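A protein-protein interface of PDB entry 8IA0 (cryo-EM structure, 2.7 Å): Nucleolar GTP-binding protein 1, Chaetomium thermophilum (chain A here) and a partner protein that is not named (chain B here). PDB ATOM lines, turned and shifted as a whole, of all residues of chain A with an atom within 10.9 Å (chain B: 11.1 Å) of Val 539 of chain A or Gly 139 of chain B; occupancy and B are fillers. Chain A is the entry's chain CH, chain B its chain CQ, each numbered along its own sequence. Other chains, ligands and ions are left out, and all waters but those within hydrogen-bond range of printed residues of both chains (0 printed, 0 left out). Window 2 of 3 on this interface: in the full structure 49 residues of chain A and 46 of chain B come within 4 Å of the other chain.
OD1 of Asp 532 of chain A is in salt-bridge range of NH2 of Arg 138 of chain B, 3.7 Å away. The side-chain carboxylate (OD2) of Asp 535 of chain A is in salt-bridge range of the guanidinium group (NH2) of Arg 138 of chain B (3.7 Å). The backbone NH (N) of Gly 139 of chain B sits at hydrogen-bond distance from the side-chain carboxylate (OD1) of Asp 535 of chain A, at 2.8 Å. The backbone NH (N) of Ser 140 of chain B is in hydrogen-bond range of the side-chain carboxylate (OD1) of Asp 535 of chain A, at 2.8 Å. NH1 of Arg 136 of chain B is in hydrogen-bond range of O of Gln 536 of chain A (2.7 Å). The side-chain amide nitrogen (NE2) of Gln 536 of chain A lies close to the guanidinium group (NH1) of Arg 138 of chain B, 3.3 Å away. The backbone carbonyl oxygen (O) of Leu 537 of chain A lies close to the guanidinium group (NH1) of Arg 136 of chain B (3.5 Å).
Among the printed residues, pairs that only touch across the chains: Val 539 of chain A with Gly 139 of chain B, Gln 536 of chain A with Leu 137 of chain B and Gly 538 of chain A with Gly 139 of chain B.
Printed residues of chain A within 4 Å of Gly 139 of chain B: Asp 535, Gly 538 and Val 539. No residue of chain B comes within 4 Å of Leu 534 of chain A. Asp 535 of chain A touches just these residues of chain B: Arg 138, Gly 139 and Ser 140. Leu 537 of chain A touches just one residue of chain B: Arg 136. Of chain B, only Gly 139 comes within 4 Å of Gly 538 of chain A. No residue of chain B comes within 4 Å of Asp 540 of chain A. No residue of chain B comes within 4 Å of Thr 541 of chain A. Of chain A, only Asp 535 comes within 4 Å of Ser 140 of chain B. No residue of chain A comes within 4 Å of Arg 143 of chain B. Printed residues of chain A within 4 Å of Leu 137 of chain B: Gln 536 (3.9 Å). Of the printed residues of chain A, Arg 138 of chain B touches Asp 532 (3.7 Å), Asp 535 (3.5 Å) and Gln 536 (3.3 Å). Printed residues of chain B within 4 Å of Asp 532 of chain A: Arg 138 (3.7 Å). Of the printed residues of chain B, Gln 536 of chain A touches Arg 136 (2.7 Å), Leu 137 (3.9 Å) and Arg 138 (3.3 Å). Of the printed residues of chain A, Arg 136 of chain B touches Gln 536 and Leu 537. His 533 of chain A touches none of the printed residues of chain B. The nearest printed residue of chain A that does not touch Leu 137 of chain B is Asp 535 of chain A (4.6 Å).
The side-chain carboxylate of Asp 532 of chain A is in hydrogen-bond range of the side-chain amide nitrogen of Gln 536 of chain A, at 2.9 Å. N of Val 539 of chain A lies within hydrogen-bond range of O of Leu 534 of chain A (3.1 Å). The backbone carbonyl oxygen of Arg 136 of chain B sits at hydrogen-bond distance from the side-chain amino group of Lys 142 of chain B, at 3.2 Å.
Printed residues of chain B that touch a printed residue of chain A: Arg 136, Leu 137, Arg 138, Gly 139 and Ser 140. Among the printed residues, 10 pairs touch across the chains.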
ATOM      1  N   SER A 528      25.144  -9.455  28.257  1.00  0.00           N
ATOM      2  CA  SER A 528      24.312 -10.654  28.270  1.00  0.00           C
ATOM      3  C   SER A 528      23.244 -10.572  29.353  1.00  0.00           C
ATOM      4  O   SER A 528      22.092 -10.964  29.136  1.00  0.00           O
ATOM      5  CB  SER A 528      25.186 -11.894  28.466  1.00  0.00           C
ATOM      6  OG  SER A 528      25.968 -11.784  29.642  1.00  0.00           O
ATOM      7  N   GLN A 529      23.611 -10.068  30.533  1.00  0.00           N
ATOM      8  CA  GLN A 529      22.635  -9.929  31.609  1.00  0.00           C
ATOM      9  C   GLN A 529      21.567  -8.900  31.261  1.00  0.00           C
ATOM     10  O   GLN A 529      20.379  -9.113  31.528  1.00  0.00           O
ATOM     11  CB  GLN A 529      23.339  -9.555  32.912  1.00  0.00           C
ATOM     12  CG  GLN A 529      24.715 -10.171  33.070  1.00  0.00           C
ATOM     13  CD  GLN A 529      25.146 -10.258  34.518  1.00  0.00           C
ATOM     14  OE1 GLN A 529      25.624 -11.297  34.975  1.00  0.00           O
ATOM     15  NE2 GLN A 529      24.983  -9.164  35.251  1.00  0.00           N
ATOM     16  N   LEU A 530      21.969  -7.772  30.670  1.00  0.00           N
ATOM     17  CA  LEU A 530      20.995  -6.758  30.286  1.00  0.00           C
ATOM     18  C   LEU A 530      20.128  -7.237  29.129  1.00  0.00           C
ATOM     19  O   LEU A 530      18.912  -7.012  29.121  1.00  0.00           O
ATOM     20  CB  LEU A 530      21.701  -5.454  29.923  1.00  0.00           C
ATOM     21  CG  LEU A 530      20.796  -4.369  29.341  1.00  0.00           C
ATOM     22  CD1 LEU A 530      19.782  -3.909  30.374  1.00  0.00           C
ATOM     23  CD2 LEU A 530      21.619  -3.199  28.844  1.00  0.00           C
ATOM     24  N   GLU A 531      20.736  -7.895  28.140  1.00  0.00           N
ATOM     25  CA  GLU A 531      19.961  -8.469  27.046  1.00  0.00           C
ATOM     26  C   GLU A 531      18.961  -9.491  27.562  1.00  0.00           C
ATOM     27  O   GLU A 531      17.799  -9.501  27.138  1.00  0.00           O
ATOM     28  CB  GLU A 531      20.898  -9.103  26.017  1.00  0.00           C
ATOM     29  CG  GLU A 531      20.368  -9.120  24.589  1.00  0.00           C
ATOM     30  CD  GLU A 531      19.594 -10.389  24.261  1.00  0.00           C
ATOM     31  OE1 GLU A 531      19.247 -11.144  25.192  1.00  0.00           O
ATOM     32  OE2 GLU A 531      19.336 -10.640  23.065  1.00  0.00           O
ATOM     33  N   ASP A 532      19.393 -10.364  28.472  1.00  0.00           N
ATOM     34  CA  ASP A 532      18.488 -11.369  29.015  1.00  0.00           C
ATOM     35  C   ASP A 532      17.346 -10.724  29.785  1.00  0.00           C
ATOM     36  O   ASP A 532      16.174 -11.013  29.525  1.00  0.00           O
ATOM     37  CB  ASP A 532      19.253 -12.341  29.910  1.00  0.00           C
ATOM     38  CG  ASP A 532      18.347 -13.087  30.867  1.00  0.00           C
ATOM     39  OD1 ASP A 532      17.505 -13.880  30.395  1.00  0.00           O
ATOM     40  OD2 ASP A 532      18.473 -12.877  32.091  1.00  0.00           O
ATOM     41  N   HIS A 533      17.667  -9.824  30.719  1.00  0.00           N
ATOM     42  CA  HIS A 533      16.640  -9.243  31.579  1.00  0.00           C
ATOM     43  C   HIS A 533      15.621  -8.449  30.777  1.00  0.00           C
ATOM     44  O   HIS A 533      14.419  -8.515  31.055  1.00  0.00           O
ATOM     45  CB  HIS A 533      17.282  -8.357  32.644  1.00  0.00           C
ATOM     46  CG  HIS A 533      16.315  -7.860  33.672  1.00  0.00           C
ATOM     47  ND1 HIS A 533      16.004  -8.574  34.808  1.00  0.00           N
ATOM     48  CD2 HIS A 533      15.579  -6.725  33.729  1.00  0.00           C
ATOM     49  CE1 HIS A 533      15.123  -7.898  35.524  1.00  0.00           C
ATOM     50  NE2 HIS A 533      14.849  -6.773  34.890  1.00  0.00           N
ATOM     51  N   LEU A 534      16.078  -7.686  29.784  1.00  0.00           N
ATOM     52  CA  LEU A 534      15.145  -6.957  28.934  1.00  0.00           C
ATOM     53  C   LEU A 534      14.249  -7.915  28.160  1.00  0.00           C
ATOM     54  O   LEU A 534      13.076  -7.616  27.909  1.00  0.00           O
ATOM     55  CB  LEU A 534      15.911  -6.044  27.978  1.00  0.00           C
ATOM     56  CG  LEU A 534      16.463  -4.749  28.576  1.00  0.00           C
ATOM     57  CD1 LEU A 534      17.039  -3.859  27.487  1.00  0.00           C
ATOM     58  CD2 LEU A 534      15.383  -4.016  29.351  1.00  0.00           C
ATOM     59  N   ASP A 535      14.786  -9.075  27.773  1.00  0.00           N
ATOM     60  CA  ASP A 535      13.987 -10.053  27.044  1.00  0.00           C
ATOM     61  C   ASP A 535      12.877 -10.631  27.917  1.00  0.00           C
ATOM     62  O   ASP A 535      11.748 -10.815  27.450  1.00  0.00           O
ATOM     63  CB  ASP A 535      14.885 -11.166  26.505  1.00  0.00           C
ATOM     64  CG  ASP A 535      14.257 -11.908  25.344  1.00  0.00           C
ATOM     65  OD1 ASP A 535      13.130 -11.547  24.945  1.00  0.00           O
ATOM     66  OD2 ASP A 535      14.890 -12.852  24.827  1.00  0.00           O
ATOM     67  N   GLN A 536      13.177 -10.929  29.185  1.00  0.00           N
ATOM     68  CA  GLN A 536      12.145 -11.449  30.079  1.00  0.00           C
ATOM     69  C   GLN A 536      11.041 -10.424  30.299  1.00  0.00           C
ATOM     70  O   GLN A 536       9.875 -10.787  30.485  1.00  0.00           O
ATOM     71  CB  GLN A 536      12.748 -11.868  31.420  1.00  0.00           C
ATOM     72  CG  GLN A 536      14.178 -12.348  31.356  1.00  0.00           C
ATOM     73  CD  GLN A 536      14.459 -13.471  32.331  1.00  0.00           C
ATOM     74  OE1 GLN A 536      14.109 -13.387  33.508  1.00  0.00           O
ATOM     75  NE2 GLN A 536      15.095 -14.531  31.847  1.00  0.00           N
ATOM     76  N   LEU A 537      11.392  -9.140  30.285  1.00  0.00           N
ATOM     77  CA  LEU A 537      10.397  -8.094  30.478  1.00  0.00           C
ATOM     78  C   LEU A 537       9.569  -7.846  29.225  1.00  0.00           C
ATOM     79  O   LEU A 537       8.615  -7.064  29.274  1.00  0.00           O
ATOM     80  CB  LEU A 537      11.079  -6.804  30.928  1.00  0.00           C
ATOM     81  CG  LEU A 537      11.824  -6.890  32.260  1.00  0.00           C
ATOM     82  CD1 LEU A 537      12.132  -5.507  32.779  1.00  0.00           C
ATOM     83  CD2 LEU A 537      11.019  -7.673  33.286  1.00  0.00           C
ATOM     84  N   GLY A 538       9.913  -8.482  28.108  1.00  0.00           N
ATOM     85  CA  GLY A 538       9.152  -8.326  26.887  1.00  0.00           C
ATOM     86  C   GLY A 538       9.613  -7.153  26.049  1.00  0.00           C
ATOM     87  O   GLY A 538       8.799  -6.334  25.615  1.00  0.00           O
ATOM     88  N   VAL A 539      10.919  -7.061  25.817  1.00  0.00           N
ATOM     89  CA  VAL A 539      11.517  -5.969  25.062  1.00  0.00           C
ATOM     90  C   VAL A 539      12.361  -6.558  23.940  1.00  0.00           C
ATOM     91  O   VAL A 539      13.098  -7.527  24.150  1.00  0.00           O
ATOM     92  CB  VAL A 539      12.368  -5.053  25.967  1.00  0.00           C
ATOM     93  CG1 VAL A 539      12.989  -3.928  25.158  1.00  0.00           C
ATOM     94  CG2 VAL A 539      11.521  -4.494  27.097  1.00  0.00           C
ATOM     95  N   ASP A 540      12.241  -5.976  22.751  1.00  0.00           N
ATOM     96  CA  ASP A 540      13.017  -6.435  21.608  1.00  0.00           C
ATOM     97  C   ASP A 540      14.497  -6.114  21.788  1.00  0.00           C
ATOM     98  O   ASP A 540      14.864  -5.071  22.333  1.00  0.00           O
ATOM     99  CB  ASP A 540      12.489  -5.801  20.323  1.00  0.00           C
ATOM    100  CG  ASP A 540      12.333  -4.297  20.435  1.00  0.00           C
ATOM    101  OD1 ASP A 540      12.506  -3.759  21.549  1.00  0.00           O
ATOM    102  OD2 ASP A 540      12.035  -3.652  19.407  1.00  0.00           O
ATOM    103  N   THR A 541      15.348  -7.029  21.325  1.00  0.00           N
ATOM    104  CA  THR A 541      16.793  -6.864  21.422  1.00  0.00           C
ATOM    105  C   THR A 541      17.346  -5.886  20.393  1.00  0.00           C
ATOM    106  O   THR A 541      18.374  -5.251  20.654  1.00  0.00           O
ATOM    107  CB  THR A 541      17.475  -8.231  21.270  1.00  0.00           C
ATOM    108  OG1 THR A 541      17.092  -9.080  22.361  1.00  0.00           O
ATOM    109  CG2 THR A 541      18.994  -8.101  21.253  1.00  0.00           C
ATOM    110  N   GLU A 542      16.664  -5.721  19.257  1.00  0.00           N
ATOM    111  CA  GLU A 542      17.159  -4.964  18.109  1.00  0.00           C
ATOM    112  C   GLU A 542      17.809  -3.631  18.473  1.00  0.00           C
ATOM    113  O   GLU A 542      18.732  -3.182  17.787  1.00  0.00           O
ATOM    114  CB  GLU A 542      16.015  -4.723  17.121  1.00  0.00           C
ATOM    115  CG  GLU A 542      14.851  -3.930  17.696  1.00  0.00           C
ATOM    116  CD  GLU A 542      15.012  -2.434  17.510  1.00  0.00           C
ATOM    117  OE1 GLU A 542      15.424  -2.011  16.410  1.00  0.00           O
ATOM    118  OE2 GLU A 542      14.735  -1.683  18.468  1.00  0.00           O
ATOM    119  N   ALA A 543      17.337  -2.990  19.544  1.00  0.00           N
ATOM    120  CA  ALA A 543      17.880  -1.690  19.926  1.00  0.00           C
ATOM    121  C   ALA A 543      19.309  -1.810  20.446  1.00  0.00           C
ATOM    122  O   ALA A 543      20.202  -1.078  20.008  1.00  0.00           O
ATOM    123  CB  ALA A 543      16.978  -1.037  20.971  1.00  0.00           C
ATOM    124  N   ILE A 544      19.545  -2.731  21.380  1.00  0.00           N
ATOM    125  CA  ILE A 544      20.844  -2.845  22.037  1.00  0.00           C
ATOM    126  C   ILE A 544      21.797  -3.665  21.180  1.00  0.00           C
ATOM    127  O   ILE A 544      21.387  -4.299  20.202  1.00  0.00           O
ATOM    128  CB  ILE A 544      20.711  -3.454  23.445  1.00  0.00           C
ATOM    129  CG1 ILE A 544      19.845  -4.713  23.408  1.00  0.00           C
ATOM    130  CG2 ILE A 544      20.136  -2.434  24.414  1.00  0.00           C
ATOM    131  CD1 ILE A 544      19.587  -5.318  24.772  1.00  0.00           C
ATOM    132  N   GLY A 545      23.077  -3.655  21.546  1.00  0.00           N
ATOM    133  CA  GLY A 545      24.103  -4.357  20.809  1.00  0.00           C
ATOM    134  C   GLY A 545      25.199  -3.475  20.253  1.00  0.00           C
ATOM    135  O   GLY A 545      26.226  -4.001  19.804  1.00  0.00           O
ATOM    136  N   ARG A 547      25.864  -0.174  21.994  1.00  0.00           N
ATOM    137  CA  ARG A 547      26.325   0.713  23.056  1.00  0.00           C
ATOM    138  C   ARG A 547      27.712   0.306  23.539  1.00  0.00           C
ATOM    139  O   ARG A 547      28.682   1.059  23.400  1.00  0.00           O
ATOM    140  CB  ARG A 547      25.321   0.708  24.211  1.00  0.00           C
ATOM    141  CG  ARG A 547      23.866   0.680  23.771  1.00  0.00           C
ATOM    142  CD  ARG A 547      23.458   1.988  23.114  1.00  0.00           C
ATOM    143  NE  ARG A 547      22.052   2.299  23.343  1.00  0.00           N
ATOM    144  CZ  ARG A 547      21.060   1.916  22.552  1.00  0.00           C
ATOM    145  NH1 ARG A 547      21.281   1.194  21.466  1.00  0.00           N
ATOM    146  NH2 ARG A 547      19.813   2.264  22.858  1.00  0.00           N
ATOM    147  N   PRO B 135       2.423 -13.344  33.656  1.00  0.00           N
ATOM    148  CA  PRO B 135       3.228 -13.858  32.540  1.00  0.00           C
ATOM    149  C   PRO B 135       3.086 -12.974  31.311  1.00  0.00           C
ATOM    150  O   PRO B 135       1.998 -12.494  30.988  1.00  0.00           O
ATOM    151  CB  PRO B 135       2.652 -15.257  32.300  1.00  0.00           C
ATOM    152  CG  PRO B 135       2.028 -15.640  33.588  1.00  0.00           C
ATOM    153  CD  PRO B 135       1.543 -14.377  34.229  1.00  0.00           C
ATOM    154  N   ARG B 136       4.210 -12.760  30.619  1.00  0.00           N
ATOM    155  CA  ARG B 136       4.252 -11.745  29.575  1.00  0.00           C
ATOM    156  C   ARG B 136       5.070 -12.216  28.367  1.00  0.00           C
ATOM    157  O   ARG B 136       5.499 -11.391  27.550  1.00  0.00           O
ATOM    158  CB  ARG B 136       4.769 -10.433  30.221  1.00  0.00           C
ATOM    159  CG  ARG B 136       5.188  -9.265  29.327  1.00  0.00           C
ATOM    160  CD  ARG B 136       5.620  -7.998  30.092  1.00  0.00           C
ATOM    161  NE  ARG B 136       5.843  -8.140  31.530  1.00  0.00           N
ATOM    162  CZ  ARG B 136       6.769  -8.904  32.097  1.00  0.00           C
ATOM    163  NH1 ARG B 136       7.619  -9.617  31.375  1.00  0.00           N
ATOM    164  NH2 ARG B 136       6.849  -8.947  33.424  1.00  0.00           N
ATOM    165  N   LEU B 137       5.250 -13.522  28.203  1.00  0.00           N
ATOM    166  CA  LEU B 137       5.982 -14.080  27.057  1.00  0.00           C
ATOM    167  C   LEU B 137       7.413 -13.536  27.087  1.00  0.00           C
ATOM    168  O   LEU B 137       7.959 -13.249  28.159  1.00  0.00           O
ATOM    169  CB  LEU B 137       5.222 -13.790  25.770  1.00  0.00           C
ATOM    170  CG  LEU B 137       5.164 -14.841  24.659  1.00  0.00           C
ATOM    171  CD1 LEU B 137       5.039 -16.239  25.227  1.00  0.00           C
ATOM    172  CD2 LEU B 137       4.016 -14.544  23.705  1.00  0.00           C
ATOM    173  N   ARG B 138       8.028 -13.392  25.916  1.00  0.00           N
ATOM    174  CA  ARG B 138       9.370 -12.841  25.809  1.00  0.00           C
ATOM    175  C   ARG B 138       9.478 -12.067  24.506  1.00  0.00           C
ATOM    176  O   ARG B 138       8.729 -12.307  23.555  1.00  0.00           O
ATOM    177  CB  ARG B 138      10.442 -13.938  25.871  1.00  0.00           C
ATOM    178  CG  ARG B 138      10.928 -14.255  27.274  1.00  0.00           C
ATOM    179  CD  ARG B 138      11.754 -15.529  27.301  1.00  0.00           C
ATOM    180  NE  ARG B 138      13.167 -15.267  27.060  1.00  0.00           N
ATOM    181  CZ  ARG B 138      14.129 -15.478  27.947  1.00  0.00           C
ATOM    182  NH1 ARG B 138      13.866 -15.958  29.151  1.00  0.00           N
ATOM    183  NH2 ARG B 138      15.387 -15.198  27.620  1.00  0.00           N
ATOM    184  N   GLY B 139      10.420 -11.124  24.475  1.00  0.00           N
ATOM    185  CA  GLY B 139      10.626 -10.346  23.264  1.00  0.00           C
ATOM    186  C   GLY B 139      11.107 -11.200  22.107  1.00  0.00           C
ATOM    187  O   GLY B 139      10.625 -11.070  20.978  1.00  0.00           O
ATOM    188  N   SER B 140      12.071 -12.084  22.371  1.00  0.00           N
ATOM    189  CA  SER B 140      12.523 -13.014  21.343  1.00  0.00           C
ATOM    190  C   SER B 140      11.420 -13.998  20.974  1.00  0.00           C
ATOM    191  O   SER B 140      11.283 -14.378  19.806  1.00  0.00           O
ATOM    192  CB  SER B 140      13.770 -13.756  21.819  1.00  0.00           C
ATOM    193  OG  SER B 140      13.475 -14.589  22.925  1.00  0.00           O
ATOM    194  N   GLU B 141      10.631 -14.430  21.960  1.00  0.00           N
ATOM    195  CA  GLU B 141       9.538 -15.355  21.684  1.00  0.00           C
ATOM    196  C   GLU B 141       8.495 -14.721  20.771  1.00  0.00           C
ATOM    197  O   GLU B 141       7.975 -15.377  19.863  1.00  0.00           O
ATOM    198  CB  GLU B 141       8.898 -15.819  22.991  1.00  0.00           C
ATOM    199  CG  GLU B 141       9.453 -17.131  23.530  1.00  0.00           C
ATOM    200  CD  GLU B 141      10.015 -18.025  22.441  1.00  0.00           C
ATOM    201  OE1 GLU B 141       9.226 -18.748  21.798  1.00  0.00           O
ATOM    202  OE2 GLU B 141      11.247 -18.014  22.236  1.00  0.00           O
ATOM    203  N   LYS B 142       8.175 -13.445  20.999  1.00  0.00           N
ATOM    204  CA  LYS B 142       7.209 -12.762  20.144  1.00  0.00           C
ATOM    205  C   LYS B 142       7.711 -12.669  18.709  1.00  0.00           C
ATOM    206  O   LYS B 142       6.942 -12.872  17.762  1.00  0.00           O
ATOM    207  CB  LYS B 142       6.908 -11.369  20.696  1.00  0.00           C
ATOM    208  CG  LYS B 142       5.652 -11.298  21.547  1.00  0.00           C
ATOM    209  CD  LYS B 142       5.422  -9.889  22.070  1.00  0.00           C
ATOM    210  CE  LYS B 142       4.639  -9.905  23.373  1.00  0.00           C
ATOM    211  NZ  LYS B 142       5.484 -10.327  24.524  1.00  0.00           N
ATOM    212  N   ARG B 143       8.995 -12.355  18.528  1.00  0.00           N
ATOM    213  CA  ARG B 143       9.559 -12.303  17.184  1.00  0.00           C
ATOM    214  C   ARG B 143       9.526 -13.676  16.525  1.00  0.00           C
ATOM    215  O   ARG B 143       9.031 -13.826  15.404  1.00  0.00           O
ATOM    216  CB  ARG B 143      10.991 -11.771  17.236  1.00  0.00           C
ATOM    217  CG  ARG B 143      11.114 -10.274  17.023  1.00  0.00           C
ATOM    218  CD  ARG B 143      12.485  -9.918  16.473  1.00  0.00           C
ATOM    219  NE  ARG B 143      13.487 -10.918  16.823  1.00  0.00           N
ATOM    220  CZ  ARG B 143      14.508 -10.704  17.640  1.00  0.00           C
ATOM    221  NH1 ARG B 143      14.698  -9.527  18.216  1.00  0.00           N
ATOM    222  NH2 ARG B 143      15.361 -11.694  17.888  1.00  0.00           N
ATOM    223  N   ARG B 144      10.041 -14.694  17.218  1.00  0.00           N
ATOM    224  CA  ARG B 144      10.093 -16.035  16.646  1.00  0.00           C
ATOM    225  C   ARG B 144       8.695 -16.572  16.367  1.00  0.00           C
ATOM    226  O   ARG B 144       8.487 -17.296  15.387  1.00  0.00           O
ATOM    227  CB  ARG B 144      10.854 -16.974  17.582  1.00  0.00           C
ATOM    228  CG  ARG B 144      11.363 -18.244  16.920  1.00  0.00           C
ATOM    229  CD  ARG B 144      10.430 -19.417  17.177  1.00  0.00           C
ATOM    230  NE  ARG B 144      10.397 -19.790  18.586  1.00  0.00           N
ATOM    231  CZ  ARG B 144       9.498 -20.601  19.126  1.00  0.00           C
ATOM    232  NH1 ARG B 144       8.536 -21.147  18.399  1.00  0.00           N
ATOM    233  NH2 ARG B 144       9.565 -20.872  20.426  1.00  0.00           N
ATOM    234  N   LEU B 145       7.729 -16.235  17.221  1.00  0.00           N
ATOM    235  CA  LEU B 145       6.355 -16.652  16.973  1.00  0.00           C
ATOM    236  C   LEU B 145       5.740 -15.879  15.813  1.00  0.00           C
ATOM    237  O   LEU B 145       4.900 -16.420  15.086  1.00  0.00           O
ATOM    238  CB  LEU B 145       5.514 -16.475  18.236  1.00  0.00           C
ATOM    239  CG  LEU B 145       5.270 -17.724  19.085  1.00  0.00           C
ATOM    240  CD1 LEU B 145       4.186 -18.587  18.472  1.00  0.00           C
ATOM    241  CD2 LEU B 145       6.551 -18.523  19.271  1.00  0.00           C
ATOM    242  N   ALA B 146       6.137 -14.617  15.632  1.00  0.00           N
ATOM    243  CA  ALA B 146       5.615 -13.829  14.520  1.00  0.00           C
ATOM    244  C   ALA B 146       6.066 -14.392  13.178  1.00  0.00           C
ATOM    245  O   ALA B 146       5.273 -14.466  12.233  1.00  0.00           O
ATOM    246  CB  ALA B 146       6.046 -12.369  14.660  1.00  0.00           C
ATOM    247  N   GLU B 147       7.338 -14.785  13.071  1.00  0.00           N
ATOM    248  CA  GLU B 147       7.810 -15.405  11.836  1.00  0.00           C
ATOM    249  C   GLU B 147       7.122 -16.741  11.596  1.00  0.00           C
ATOM    250  O   GLU B 147       6.763 -17.068  10.460  1.00  0.00           O
ATOM    251  CB  GLU B 147       9.331 -15.583  11.871  1.00  0.00           C
ATOM    252  CG  GLU B 147      10.166 -14.507  12.605  1.00  0.00           C
ATOM    253  CD  GLU B 147       9.847 -13.043  12.265  1.00  0.00           C
ATOM    254  OE1 GLU B 147       8.885 -12.740  11.528  1.00  0.00           O
ATOM    255  OE2 GLU B 147      10.591 -12.171  12.760  1.00  0.00           O
ATOM    256  N   VAL B 156      -2.010 -15.059  14.823  1.00  0.00           N
ATOM    257  CA  VAL B 156      -0.878 -14.802  15.706  1.00  0.00           C
ATOM    258  C   VAL B 156      -1.337 -14.708  17.157  1.00  0.00           C
ATOM    259  O   VAL B 156      -0.628 -15.142  18.073  1.00  0.00           O
ATOM    260  CB  VAL B 156      -0.121 -13.537  15.255  1.00  0.00           C
ATOM    261  CG1 VAL B 156      -0.976 -12.288  15.430  1.00  0.00           C
ATOM    262  CG2 VAL B 156       1.192 -13.404  16.012  1.00  0.00           C
ATOM    263  N   GLU B 160       0.050 -17.102  19.975  1.00  0.00           N
ATOM    264  CA  GLU B 160       0.693 -16.566  21.170  1.00  0.00           C
ATOM    265  C   GLU B 160       0.056 -17.119  22.438  1.00  0.00           C
ATOM    266  O   GLU B 160       0.760 -17.467  23.394  1.00  0.00           O
ATOM    267  CB  GLU B 160       0.629 -15.039  21.165  1.00  0.00           C
ATOM    268  CG  GLU B 160       1.658 -14.371  20.267  1.00  0.00           C
ATOM    269  CD  GLU B 160       1.228 -12.988  19.819  1.00  0.00           C
ATOM    270  OE1 GLU B 160       0.141 -12.538  20.238  1.00  0.00           O
ATOM    271  OE2 GLU B 160       1.978 -12.350  19.050  1.00  0.00           O
ATOM    272  N   GLU B 163       1.261 -20.585  23.123  1.00  0.00           N
ATOM    273  CA  GLU B 163       2.617 -20.547  23.659  1.00  0.00           C
ATOM    274  C   GLU B 163       2.625 -20.062  25.103  1.00  0.00           C
ATOM    275  O   GLU B 163       3.384 -20.572  25.934  1.00  0.00           O
ATOM    276  CB  GLU B 163       3.501 -19.656  22.788  1.00  0.00           C
ATOM    277  CG  GLU B 163       4.955 -19.598  23.230  1.00  0.00           C
ATOM    278  CD  GLU B 163       5.689 -20.905  23.002  1.00  0.00           C
ATOM    279  OE1 GLU B 163       5.303 -21.652  22.080  1.00  0.00           O
ATOM    280  OE2 GLU B 163       6.652 -21.184  23.747  1.00  0.00           O
ATOM    281  N   LEU B 164       1.791 -19.069  25.418  1.00  0.00           N
ATOM    282  CA  LEU B 164       1.739 -18.549  26.780  1.00  0.00           C
ATOM    283  C   LEU B 164       1.266 -19.615  27.761  1.00  0.00           C
ATOM    284  O   LEU B 164       1.796 -19.727  28.872  1.00  0.00           O
ATOM    285  CB  LEU B 164       0.827 -17.324  26.835  1.00  0.00           C
ATOM    286  CG  LEU B 164       0.745 -16.574  28.167  1.00  0.00           C
ATOM    287  CD1 LEU B 164       2.127 -16.412  28.786  1.00  0.00           C
ATOM    288  CD2 LEU B 164       0.078 -15.222  27.975  1.00  0.00           C
ATOM    289  N   LEU B 167       4.041 -22.593  28.388  1.00  0.00           N
ATOM    290  CA  LEU B 167       5.146 -22.253  29.279  1.00  0.00           C
ATOM    291  C   LEU B 167       4.676 -22.117  30.721  1.00  0.00           C
ATOM    292  O   LEU B 167       5.412 -22.479  31.647  1.00  0.00           O
ATOM    293  CB  LEU B 167       5.837 -20.969  28.812  1.00  0.00           C
ATOM    294  CG  LEU B 167       5.080 -19.639  28.829  1.00  0.00           C
ATOM    295  CD1 LEU B 167       5.323 -18.873  30.123  1.00  0.00           C
ATOM    296  CD2 LEU B 167       5.493 -18.803  27.637  1.00  0.00           C
